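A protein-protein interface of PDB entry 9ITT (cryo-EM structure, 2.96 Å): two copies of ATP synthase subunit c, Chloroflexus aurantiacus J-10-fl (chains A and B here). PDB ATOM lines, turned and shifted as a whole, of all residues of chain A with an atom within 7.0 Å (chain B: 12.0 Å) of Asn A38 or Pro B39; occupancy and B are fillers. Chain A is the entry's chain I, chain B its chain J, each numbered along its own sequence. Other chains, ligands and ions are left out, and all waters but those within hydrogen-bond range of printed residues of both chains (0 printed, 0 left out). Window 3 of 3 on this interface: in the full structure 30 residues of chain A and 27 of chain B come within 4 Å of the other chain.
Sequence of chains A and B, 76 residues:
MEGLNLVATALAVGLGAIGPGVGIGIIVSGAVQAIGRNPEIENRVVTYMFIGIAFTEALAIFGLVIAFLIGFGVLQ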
ATOM      1  N   ALA A  31     -10.765  29.145 -37.423  1.00  0.00           N
ATOM      2  CA  ALA A  31     -12.140  29.551 -37.156  1.00  0.00           C
ATOM      3  C   ALA A  31     -13.122  28.754 -38.002  1.00  0.00           C
ATOM      4  O   ALA A  31     -14.175  28.334 -37.512  1.00  0.00           O
ATOM      5  CB  ALA A  31     -12.302  31.048 -37.410  1.00  0.00           C
ATOM      6  N   VAL A  32     -12.791  28.529 -39.273  1.00  0.00           N
ATOM      7  CA  VAL A  32     -13.683  27.788 -40.157  1.00  0.00           C
ATOM      8  C   VAL A  32     -13.810  26.342 -39.697  1.00  0.00           C
ATOM      9  O   VAL A  32     -14.905  25.766 -39.712  1.00  0.00           O
ATOM     10  CB  VAL A  32     -13.179  27.893 -41.608  1.00  0.00           C
ATOM     11  CG1 VAL A  32     -13.858  26.879 -42.500  1.00  0.00           C
ATOM     12  CG2 VAL A  32     -13.408  29.298 -42.146  1.00  0.00           C
ATOM     13  N   GLN A  33     -12.697  25.722 -39.303  1.00  0.00           N
ATOM     14  CA  GLN A  33     -12.765  24.350 -38.813  1.00  0.00           C
ATOM     15  C   GLN A  33     -13.598  24.268 -37.538  1.00  0.00           C
ATOM     16  O   GLN A  33     -14.402  23.340 -37.369  1.00  0.00           O
ATOM     17  CB  GLN A  33     -11.356  23.807 -38.583  1.00  0.00           C
ATOM     18  CG  GLN A  33     -10.598  23.503 -39.871  1.00  0.00           C
ATOM     19  CD  GLN A  33      -9.642  22.334 -39.729  1.00  0.00           C
ATOM     20  OE1 GLN A  33     -10.063  21.192 -39.548  1.00  0.00           O
ATOM     21  NE2 GLN A  33      -8.347  22.615 -39.814  1.00  0.00           N
ATOM     22  N   ALA A  34     -13.434  25.240 -36.636  1.00  0.00           N
ATOM     23  CA  ALA A  34     -14.250  25.263 -35.426  1.00  0.00           C
ATOM     24  C   ALA A  34     -15.728  25.423 -35.762  1.00  0.00           C
ATOM     25  O   ALA A  34     -16.587  24.780 -35.147  1.00  0.00           O
ATOM     26  CB  ALA A  34     -13.785  26.387 -34.502  1.00  0.00           C
ATOM     27  N   ILE A  35     -16.043  26.284 -36.735  1.00  0.00           N
ATOM     28  CA  ILE A  35     -17.430  26.461 -37.161  1.00  0.00           C
ATOM     29  C   ILE A  35     -17.983  25.150 -37.702  1.00  0.00           C
ATOM     30  O   ILE A  35     -19.121  24.764 -37.408  1.00  0.00           O
ATOM     31  CB  ILE A  35     -17.526  27.584 -38.212  1.00  0.00           C
ATOM     32  CG1 ILE A  35     -17.263  28.958 -37.583  1.00  0.00           C
ATOM     33  CG2 ILE A  35     -18.889  27.564 -38.901  1.00  0.00           C
ATOM     34  CD1 ILE A  35     -18.365  29.479 -36.694  1.00  0.00           C
ATOM     35  N   GLY A  36     -17.188  24.455 -38.515  1.00  0.00           N
ATOM     36  CA  GLY A  36     -17.614  23.162 -39.023  1.00  0.00           C
ATOM     37  C   GLY A  36     -17.880  22.167 -37.912  1.00  0.00           C
ATOM     38  O   GLY A  36     -18.815  21.366 -37.992  1.00  0.00           O
ATOM     39  N   ARG A  37     -17.060  22.202 -36.858  1.00  0.00           N
ATOM     40  CA  ARG A  37     -17.273  21.326 -35.712  1.00  0.00           C
ATOM     41  C   ARG A  37     -18.290  21.874 -34.718  1.00  0.00           C
ATOM     42  O   ARG A  37     -18.758  21.120 -33.859  1.00  0.00           O
ATOM     43  CB  ARG A  37     -15.951  21.077 -34.985  1.00  0.00           C
ATOM     44  CG  ARG A  37     -15.051  20.067 -35.673  1.00  0.00           C
ATOM     45  CD  ARG A  37     -13.893  19.662 -34.778  1.00  0.00           C
ATOM     46  NE  ARG A  37     -12.681  19.404 -35.548  1.00  0.00           N
ATOM     47  CZ  ARG A  37     -11.441  19.574 -35.103  1.00  0.00           C
ATOM     48  NH1 ARG A  37     -11.192  19.970 -33.864  1.00  0.00           N
ATOM     49  NH2 ARG A  37     -10.421  19.335 -35.923  1.00  0.00           N
ATOM     50  N   ASN A  38     -18.643  23.158 -34.805  1.00  0.00           N
ATOM     51  CA  ASN A  38     -19.557  23.749 -33.833  1.00  0.00           C
ATOM     52  C   ASN A  38     -20.200  25.015 -34.389  1.00  0.00           C
ATOM     53  O   ASN A  38     -19.717  26.122 -34.123  1.00  0.00           O
ATOM     54  CB  ASN A  38     -18.815  24.062 -32.531  1.00  0.00           C
ATOM     55  CG  ASN A  38     -19.751  24.461 -31.404  1.00  0.00           C
ATOM     56  OD1 ASN A  38     -20.463  25.461 -31.496  1.00  0.00           O
ATOM     57  ND2 ASN A  38     -19.752  23.680 -30.331  1.00  0.00           N
ATOM     58  N   PRO A  39     -21.280  24.902 -35.169  1.00  0.00           N
ATOM     59  CA  PRO A  39     -21.975  26.116 -35.629  1.00  0.00           C
ATOM     60  C   PRO A  39     -22.630  26.914 -34.512  1.00  0.00           C
ATOM     61  O   PRO A  39     -22.971  28.082 -34.733  1.00  0.00           O
ATOM     62  CB  PRO A  39     -23.024  25.576 -36.613  1.00  0.00           C
ATOM     63  CG  PRO A  39     -22.559  24.207 -36.979  1.00  0.00           C
ATOM     64  CD  PRO A  39     -21.832  23.684 -35.785  1.00  0.00           C
ATOM     65  N   GLU A  40     -22.826  26.330 -33.327  1.00  0.00           N
ATOM     66  CA  GLU A  40     -23.591  26.999 -32.280  1.00  0.00           C
ATOM     67  C   GLU A  40     -22.775  28.034 -31.511  1.00  0.00           C
ATOM     68  O   GLU A  40     -23.345  28.753 -30.681  1.00  0.00           O
ATOM     69  CB  GLU A  40     -24.155  25.964 -31.307  1.00  0.00           C
ATOM     70  CG  GLU A  40     -25.512  26.335 -30.733  1.00  0.00           C
ATOM     71  CD  GLU A  40     -26.641  26.159 -31.733  1.00  0.00           C
ATOM     72  OE1 GLU A  40     -26.379  25.676 -32.855  1.00  0.00           O
ATOM     73  OE2 GLU A  40     -27.792  26.506 -31.396  1.00  0.00           O
ATOM     74  N   ILE A  41     -21.469  28.125 -31.758  1.00  0.00           N
ATOM     75  CA  ILE A  41     -20.588  29.069 -31.074  1.00  0.00           C
ATOM     76  C   ILE A  41     -20.101  30.086 -32.104  1.00  0.00           C
ATOM     77  O   ILE A  41     -18.991  30.628 -32.000  1.00  0.00           O
ATOM     78  CB  ILE A  41     -19.432  28.317 -30.378  1.00  0.00           C
ATOM     79  CG1 ILE A  41     -18.715  29.195 -29.340  1.00  0.00           C
ATOM     80  CG2 ILE A  41     -18.450  27.749 -31.403  1.00  0.00           C
ATOM     81  CD1 ILE A  41     -19.578  29.608 -28.160  1.00  0.00           C
ATOM     82  N   GLU A  42     -20.954  30.355 -33.096  1.00  0.00           N
ATOM     83  CA  GLU A  42     -20.534  31.046 -34.310  1.00  0.00           C
ATOM     84  C   GLU A  42     -20.061  32.466 -34.028  1.00  0.00           C
ATOM     85  O   GLU A  42     -18.917  32.822 -34.323  1.00  0.00           O
ATOM     86  CB  GLU A  42     -21.688  31.055 -35.315  1.00  0.00           C
ATOM     87  CG  GLU A  42     -21.401  31.826 -36.601  1.00  0.00           C
ATOM     88  CD  GLU A  42     -22.224  31.347 -37.789  1.00  0.00           C
ATOM     89  OE1 GLU A  42     -22.889  30.295 -37.691  1.00  0.00           O
ATOM     90  OE2 GLU A  42     -22.206  32.031 -38.833  1.00  0.00           O
ATOM     91  N   VAL A  45     -16.927  32.739 -31.631  1.00  0.00           N
ATOM     92  CA  VAL A  45     -15.612  32.485 -32.219  1.00  0.00           C
ATOM     93  C   VAL A  45     -15.303  33.481 -33.336  1.00  0.00           C
ATOM     94  O   VAL A  45     -14.130  33.761 -33.610  1.00  0.00           O
ATOM     95  CB  VAL A  45     -15.485  31.037 -32.726  1.00  0.00           C
ATOM     96  CG1 VAL A  45     -15.683  30.054 -31.580  1.00  0.00           C
ATOM     97  CG2 VAL A  45     -16.441  30.759 -33.884  1.00  0.00           C
ATOM     98  N   SER B  29      -5.832  30.365 -33.980  1.00  0.00           N
ATOM     99  CA  SER B  29      -6.387  29.139 -34.541  1.00  0.00           C
ATOM    100  C   SER B  29      -6.559  28.076 -33.464  1.00  0.00           C
ATOM    101  O   SER B  29      -7.625  27.459 -33.349  1.00  0.00           O
ATOM    102  CB  SER B  29      -5.491  28.626 -35.668  1.00  0.00           C
ATOM    103  OG  SER B  29      -5.916  27.353 -36.120  1.00  0.00           O
ATOM    104  N   GLY B  30      -5.522  27.857 -32.652  1.00  0.00           N
ATOM    105  CA  GLY B  30      -5.633  26.879 -31.583  1.00  0.00           C
ATOM    106  C   GLY B  30      -6.693  27.252 -30.564  1.00  0.00           C
ATOM    107  O   GLY B  30      -7.454  26.396 -30.102  1.00  0.00           O
ATOM    108  N   ALA B  31      -6.762  28.535 -30.203  1.00  0.00           N
ATOM    109  CA  ALA B  31      -7.739  28.978 -29.216  1.00  0.00           C
ATOM    110  C   ALA B  31      -9.160  28.782 -29.723  1.00  0.00           C
ATOM    111  O   ALA B  31     -10.032  28.302 -28.991  1.00  0.00           O
ATOM    112  CB  ALA B  31      -7.491  30.443 -28.858  1.00  0.00           C
ATOM    113  N   VAL B  32      -9.414  29.143 -30.982  1.00  0.00           N
ATOM    114  CA  VAL B  32     -10.753  28.987 -31.533  1.00  0.00           C
ATOM    115  C   VAL B  32     -11.095  27.512 -31.694  1.00  0.00           C
ATOM    116  O   VAL B  32     -12.246  27.107 -31.506  1.00  0.00           O
ATOM    117  CB  VAL B  32     -10.881  29.749 -32.863  1.00  0.00           C
ATOM    118  CG1 VAL B  32     -12.221  29.449 -33.502  1.00  0.00           C
ATOM    119  CG2 VAL B  32     -10.729  31.248 -32.637  1.00  0.00           C
ATOM    120  N   GLN B  33     -10.109  26.685 -32.055  1.00  0.00           N
ATOM    121  CA  GLN B  33     -10.356  25.250 -32.135  1.00  0.00           C
ATOM    122  C   GLN B  33     -10.755  24.692 -30.775  1.00  0.00           C
ATOM    123  O   GLN B  33     -11.707  23.910 -30.668  1.00  0.00           O
ATOM    124  CB  GLN B  33      -9.114  24.534 -32.664  1.00  0.00           C
ATOM    125  CG  GLN B  33      -9.387  23.163 -33.258  1.00  0.00           C
ATOM    126  CD  GLN B  33     -10.131  23.236 -34.576  1.00  0.00           C
ATOM    127  OE1 GLN B  33     -11.314  22.907 -34.655  1.00  0.00           O
ATOM    128  NE2 GLN B  33      -9.438  23.670 -35.621  1.00  0.00           N
ATOM    129  N   ALA B  34     -10.040  25.093 -29.720  1.00  0.00           N
ATOM    130  CA  ALA B  34     -10.391  24.641 -28.379  1.00  0.00           C
ATOM    131  C   ALA B  34     -11.773  25.141 -27.975  1.00  0.00           C
ATOM    132  O   ALA B  34     -12.556  24.402 -27.365  1.00  0.00           O
ATOM    133  CB  ALA B  34      -9.337  25.110 -27.376  1.00  0.00           C
ATOM    134  N   ILE B  35     -12.089  26.395 -28.305  1.00  0.00           N
ATOM    135  CA  ILE B  35     -13.391  26.957 -27.951  1.00  0.00           C
ATOM    136  C   ILE B  35     -14.507  26.192 -28.649  1.00  0.00           C
ATOM    137  O   ILE B  35     -15.536  25.873 -28.040  1.00  0.00           O
ATOM    138  CB  ILE B  35     -13.432  28.459 -28.290  1.00  0.00           C
ATOM    139  CG1 ILE B  35     -12.524  29.241 -27.336  1.00  0.00           C
ATOM    140  CG2 ILE B  35     -14.863  28.989 -28.212  1.00  0.00           C
ATOM    141  CD1 ILE B  35     -12.127  30.613 -27.847  1.00  0.00           C
ATOM    142  N   GLY B  36     -14.329  25.892 -29.936  1.00  0.00           N
ATOM    143  CA  GLY B  36     -15.303  25.067 -30.630  1.00  0.00           C
ATOM    144  C   GLY B  36     -15.430  23.691 -30.005  1.00  0.00           C
ATOM    145  O   GLY B  36     -16.535  23.160 -29.870  1.00  0.00           O
ATOM    146  N   ARG B  37     -14.301  23.098 -29.616  1.00  0.00           N
ATOM    147  CA  ARG B  37     -14.347  21.830 -28.897  1.00  0.00           C
ATOM    148  C   ARG B  37     -14.986  21.997 -27.524  1.00  0.00           C
ATOM    149  O   ARG B  37     -15.772  21.147 -27.090  1.00  0.00           O
ATOM    150  CB  ARG B  37     -12.938  21.254 -28.756  1.00  0.00           C
ATOM    151  CG  ARG B  37     -12.371  20.665 -30.034  1.00  0.00           C
ATOM    152  CD  ARG B  37     -11.164  19.790 -29.744  1.00  0.00           C
ATOM    153  NE  ARG B  37     -10.152  19.886 -30.795  1.00  0.00           N
ATOM    154  CZ  ARG B  37      -8.963  20.470 -30.682  1.00  0.00           C
ATOM    155  NH1 ARG B  37      -8.579  21.075 -29.567  1.00  0.00           N
ATOM    156  NH2 ARG B  37      -8.135  20.453 -31.722  1.00  0.00           N
ATOM    157  N   ASN B  38     -14.663  23.086 -26.827  1.00  0.00           N
ATOM    158  CA  ASN B  38     -15.092  23.278 -25.441  1.00  0.00           C
ATOM    159  C   ASN B  38     -15.467  24.738 -25.235  1.00  0.00           C
ATOM    160  O   ASN B  38     -14.667  25.535 -24.726  1.00  0.00           O
ATOM    161  CB  ASN B  38     -14.000  22.856 -24.461  1.00  0.00           C
ATOM    162  CG  ASN B  38     -14.501  22.753 -23.033  1.00  0.00           C
ATOM    163  OD1 ASN B  38     -15.306  23.567 -22.580  1.00  0.00           O
ATOM    164  ND2 ASN B  38     -14.016  21.751 -22.310  1.00  0.00           N
ATOM    165  N   PRO B  39     -16.685  25.132 -25.621  1.00  0.00           N
ATOM    166  CA  PRO B  39     -17.128  26.507 -25.331  1.00  0.00           C
ATOM    167  C   PRO B  39     -17.309  26.791 -23.849  1.00  0.00           C
ATOM    168  O   PRO B  39     -17.390  27.966 -23.469  1.00  0.00           O
ATOM    169  CB  PRO B  39     -18.464  26.618 -26.084  1.00  0.00           C
ATOM    170  CG  PRO B  39     -18.469  25.486 -27.060  1.00  0.00           C
ATOM    171  CD  PRO B  39     -17.677  24.396 -26.423  1.00  0.00           C
ATOM    172  N   GLU B  40     -17.375  25.760 -23.003  1.00  0.00           N
ATOM    173  CA  GLU B  40     -17.688  25.959 -21.592  1.00  0.00           C
ATOM    174  C   GLU B  40     -16.570  26.657 -20.829  1.00  0.00           C
ATOM    175  O   GLU B  40     -16.845  27.290 -19.804  1.00  0.00           O
ATOM    176  CB  GLU B  40     -17.997  24.612 -20.937  1.00  0.00           C
ATOM    177  CG  GLU B  40     -18.659  24.720 -19.574  1.00  0.00           C
ATOM    178  CD  GLU B  40     -18.968  23.364 -18.970  1.00  0.00           C
ATOM    179  OE1 GLU B  40     -18.654  22.340 -19.613  1.00  0.00           O
ATOM    180  OE2 GLU B  40     -19.523  23.322 -17.852  1.00  0.00           O
ATOM    181  N   ILE B  41     -15.326  26.559 -21.299  1.00  0.00           N
ATOM    182  CA  ILE B  41     -14.181  27.170 -20.625  1.00  0.00           C
ATOM    183  C   ILE B  41     -13.669  28.316 -21.485  1.00  0.00           C
ATOM    184  O   ILE B  41     -12.461  28.580 -21.530  1.00  0.00           O
ATOM    185  CB  ILE B  41     -13.066  26.142 -20.345  1.00  0.00           C
ATOM    186  CG1 ILE B  41     -12.590  25.472 -21.639  1.00  0.00           C
ATOM    187  CG2 ILE B  41     -13.554  25.092 -19.356  1.00  0.00           C
ATOM    188  CD1 ILE B  41     -11.434  24.519 -21.442  1.00  0.00           C
ATOM    189  N   GLU B  42     -14.587  28.986 -22.189  1.00  0.00           N
ATOM    190  CA  GLU B  42     -14.202  30.005 -23.160  1.00  0.00           C
ATOM    191  C   GLU B  42     -13.332  31.081 -22.520  1.00  0.00           C
ATOM    192  O   GLU B  42     -12.264  31.415 -23.039  1.00  0.00           O
ATOM    193  CB  GLU B  42     -15.460  30.612 -23.789  1.00  0.00           C
ATOM    194  CG  GLU B  42     -15.278  31.969 -24.467  1.00  0.00           C
ATOM    195  CD  GLU B  42     -16.550  32.455 -25.126  1.00  0.00           C
ATOM    196  OE1 GLU B  42     -17.427  31.620 -25.426  1.00  0.00           O
ATOM    197  OE2 GLU B  42     -16.678  33.679 -25.336  1.00  0.00           O
ATOM    198  N   ASN B  43     -13.766  31.627 -21.383  1.00  0.00           N
ATOM    199  CA  ASN B  43     -12.983  32.671 -20.730  1.00  0.00           C
ATOM    200  C   ASN B  43     -11.624  32.145 -20.282  1.00  0.00           C
ATOM    201  O   ASN B  43     -10.607  32.838 -20.409  1.00  0.00           O
ATOM    202  CB  ASN B  43     -13.758  33.239 -19.540  1.00  0.00           C
ATOM    203  CG  ASN B  43     -14.971  34.042 -19.967  1.00  0.00           C
ATOM    204  OD1 ASN B  43     -14.879  34.916 -20.828  1.00  0.00           O
ATOM    205  ND2 ASN B  43     -16.118  33.752 -19.362  1.00  0.00           N
ATOM    206  N   ARG B  44     -11.590  30.917 -19.757  1.00  0.00           N
ATOM    207  CA  ARG B  44     -10.340  30.359 -19.250  1.00  0.00           C
ATOM    208  C   ARG B  44      -9.299  30.243 -20.356  1.00  0.00           C
ATOM    209  O   ARG B  44      -8.159  30.695 -20.194  1.00  0.00           O
ATOM    210  CB  ARG B  44     -10.607  28.993 -18.614  1.00  0.00           C
ATOM    211  CG  ARG B  44      -9.386  28.304 -18.002  1.00  0.00           C
ATOM    212  CD  ARG B  44      -8.741  29.131 -16.898  1.00  0.00           C
ATOM    213  NE  ARG B  44      -9.698  29.503 -15.861  1.00  0.00           N
ATOM    214  CZ  ARG B  44     -10.144  28.684 -14.916  1.00  0.00           C
ATOM    215  NH1 ARG B  44      -9.753  27.420 -14.848  1.00  0.00           N
ATOM    216  NH2 ARG B  44     -11.010  29.144 -14.017  1.00  0.00           N
ATOM    217  N   VAL B  45      -9.670  29.645 -21.489  1.00  0.00           N
ATOM    218  CA  VAL B  45      -8.726  29.510 -22.594  1.00  0.00           C
ATOM    219  C   VAL B  45      -8.435  30.865 -23.231  1.00  0.00           C
ATOM    220  O   VAL B  45      -7.320  31.103 -23.708  1.00  0.00           O
ATOM    221  CB  VAL B  45      -9.246  28.502 -23.636  1.00  0.00           C
ATOM    222  CG1 VAL B  45      -9.454  27.134 -23.000  1.00  0.00           C
ATOM    223  CG2 VAL B  45     -10.534  28.995 -24.300  1.00  0.00           C
ATOM    224  N   VAL B  46      -9.417  31.767 -23.261  1.00  0.00           N
ATOM    225  CA  VAL B  46      -9.221  33.065 -23.896  1.00  0.00           C
ATOM    226  C   VAL B  46      -8.249  33.931 -23.099  1.00  0.00           C
ATOM    227  O   VAL B  46      -7.552  34.777 -23.672  1.00  0.00           O
ATOM    228  CB  VAL B  46     -10.586  33.753 -24.100  1.00  0.00           C
ATOM    229  CG1 VAL B  46     -10.412  35.211 -24.450  1.00  0.00           C
ATOM    230  CG2 VAL B  46     -11.357  33.062 -25.219  1.00  0.00           C
ATOM    231  N   THR B  47      -8.182  33.752 -21.777  1.00  0.00           N
ATOM    232  CA  THR B  47      -7.165  34.457 -20.997  1.00  0.00           C
ATOM    233  C   THR B  47      -5.762  34.050 -21.440  1.00  0.00           C
ATOM    234  O   THR B  47      -4.891  34.902 -21.681  1.00  0.00           O
ATOM    235  CB  THR B  47      -7.358  34.173 -19.505  1.00  0.00           C
ATOM    236  OG1 THR B  47      -8.711  34.457 -19.128  1.00  0.00           O
ATOM    237  CG2 THR B  47      -6.410  35.022 -18.668  1.00  0.00           C
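The guanidinium group (NE) of Arg B37 lies close to the guanidinium group (NH1) of Arg A37 (3.2 Å).
The side-chain amide oxygen of Gln B33 lies within hydrogen-bond range of the guanidinium group of Arg A37.
The side-chain amide nitrogen (ND2) of Asn A38 lies within hydrogen-bond range of the backbone carbonyl oxygen (O) of Gly B36, at 3.3 Å.
Val B32 touches Ala A31 (CG1 to CA, 3.7 Å).
Gln A33 touches Gln B33.
Ala A34 touches Val B32 (CB to O, 3.4 Å).
Gln B33 touches Ala A34 (OE1 to N, 3.7 Å).
Pro B39 touches Asn A38 (CG to ND2, 3.95 Å).
Pro B39 touches Ile A41.
CG1 of Val B32 touches CB of Val A45, 3.7 Å away.
Ile B35 touches Val A45.
Hydrophobic or aromatic side chains of chain A within 4 Å of the printed part of chain B: Ala A34, Ile A41 and Val A45.
Of the 19 printed residues of chain B, 6 touch a printed residue of chain A.
Hydrophobic or aromatic side chains of chain B that line the printed part of chain A: Val B32, Ile B35 and Pro B39.
Among the printed residues, 11 pairs touch across the chains.
Among the printed residues, no Asp or Glu carboxylate lies within 4 Å of a Lys or Arg side-chain nitrogen of the other chain.
Printed residues of chain B within 4 Å of Gln A33: Gln B33 (3.5 Å).
Printed residues of chain B within 4 Å of Ala A34: Val B32 (3.4 Å) and Gln B33 (3.7 Å).
No residue of chain B comes within 4 Å of Ile A35.
No residue of chain B comes within 4 Å of Gly A36.
Asn A38 touches just these residues of chain B: Gly B36 and Pro B39.
No residue of chain B comes within 4 Å of Pro A39.
Of the printed residues of chain B, Val A45 touches Val B32 and Ile B35.
Printed residues of chain A within 4 Å of Val B32: Ala A31 (3.7 Å), Ala A34 (3.4 Å) and Val A45 (3.7 Å).
Ala B34 touches none of the printed residues of chain A.
Printed residues of chain A within 4 Å of Ile B35: Val A45 (3.6 Å).
Printed residues of chain A within 4 Å of Arg B37: Arg A37.
Pro B39 touches two residues of chain A.
Arg B44 touches none of the printed residues of chain A.
The nearest residue of chain B that does not touch Asn A38 is Ile B35 (5.3 Å).
The nearest residue of chain A that does not touch Pro B39 is Glu A40 (6.7 Å).
The nearest printed residue of chain A that does not touch Arg B37 is Asn A38 (5.5 Å).
Gln B33 touches its own counterpart, Gln A33.
Ala A34 touches Gln B33, but with the chains exchanged Gln A33 does not touch Ala B34 (8.6 Å).
Arg A37 touches Gln B33, but with the chains exchanged Gln A33 does not touch Arg B37 (7.8 Å).
Asn A38 touches Pro B39, but with the chains exchanged Pro A39 does not touch Asn B38 (10.8 Å).
Positions printed for both chains: 31, 32, 33, 34, 35, 36, 37, 38, 39, 40, 41, 42 and 45.
Of the 11 pairs that touch across the chains among the printed residues, 2 have their exchanged pair printed and touching as well.
The side-chain amide oxygen (OD1) of Asn A38 is in hydrogen-bond range of the backbone NH (N) of Glu A40 (3.1 Å).
OD1 of Asn A38 is in hydrogen-bond range of N of Ile A41 (2.9 Å).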
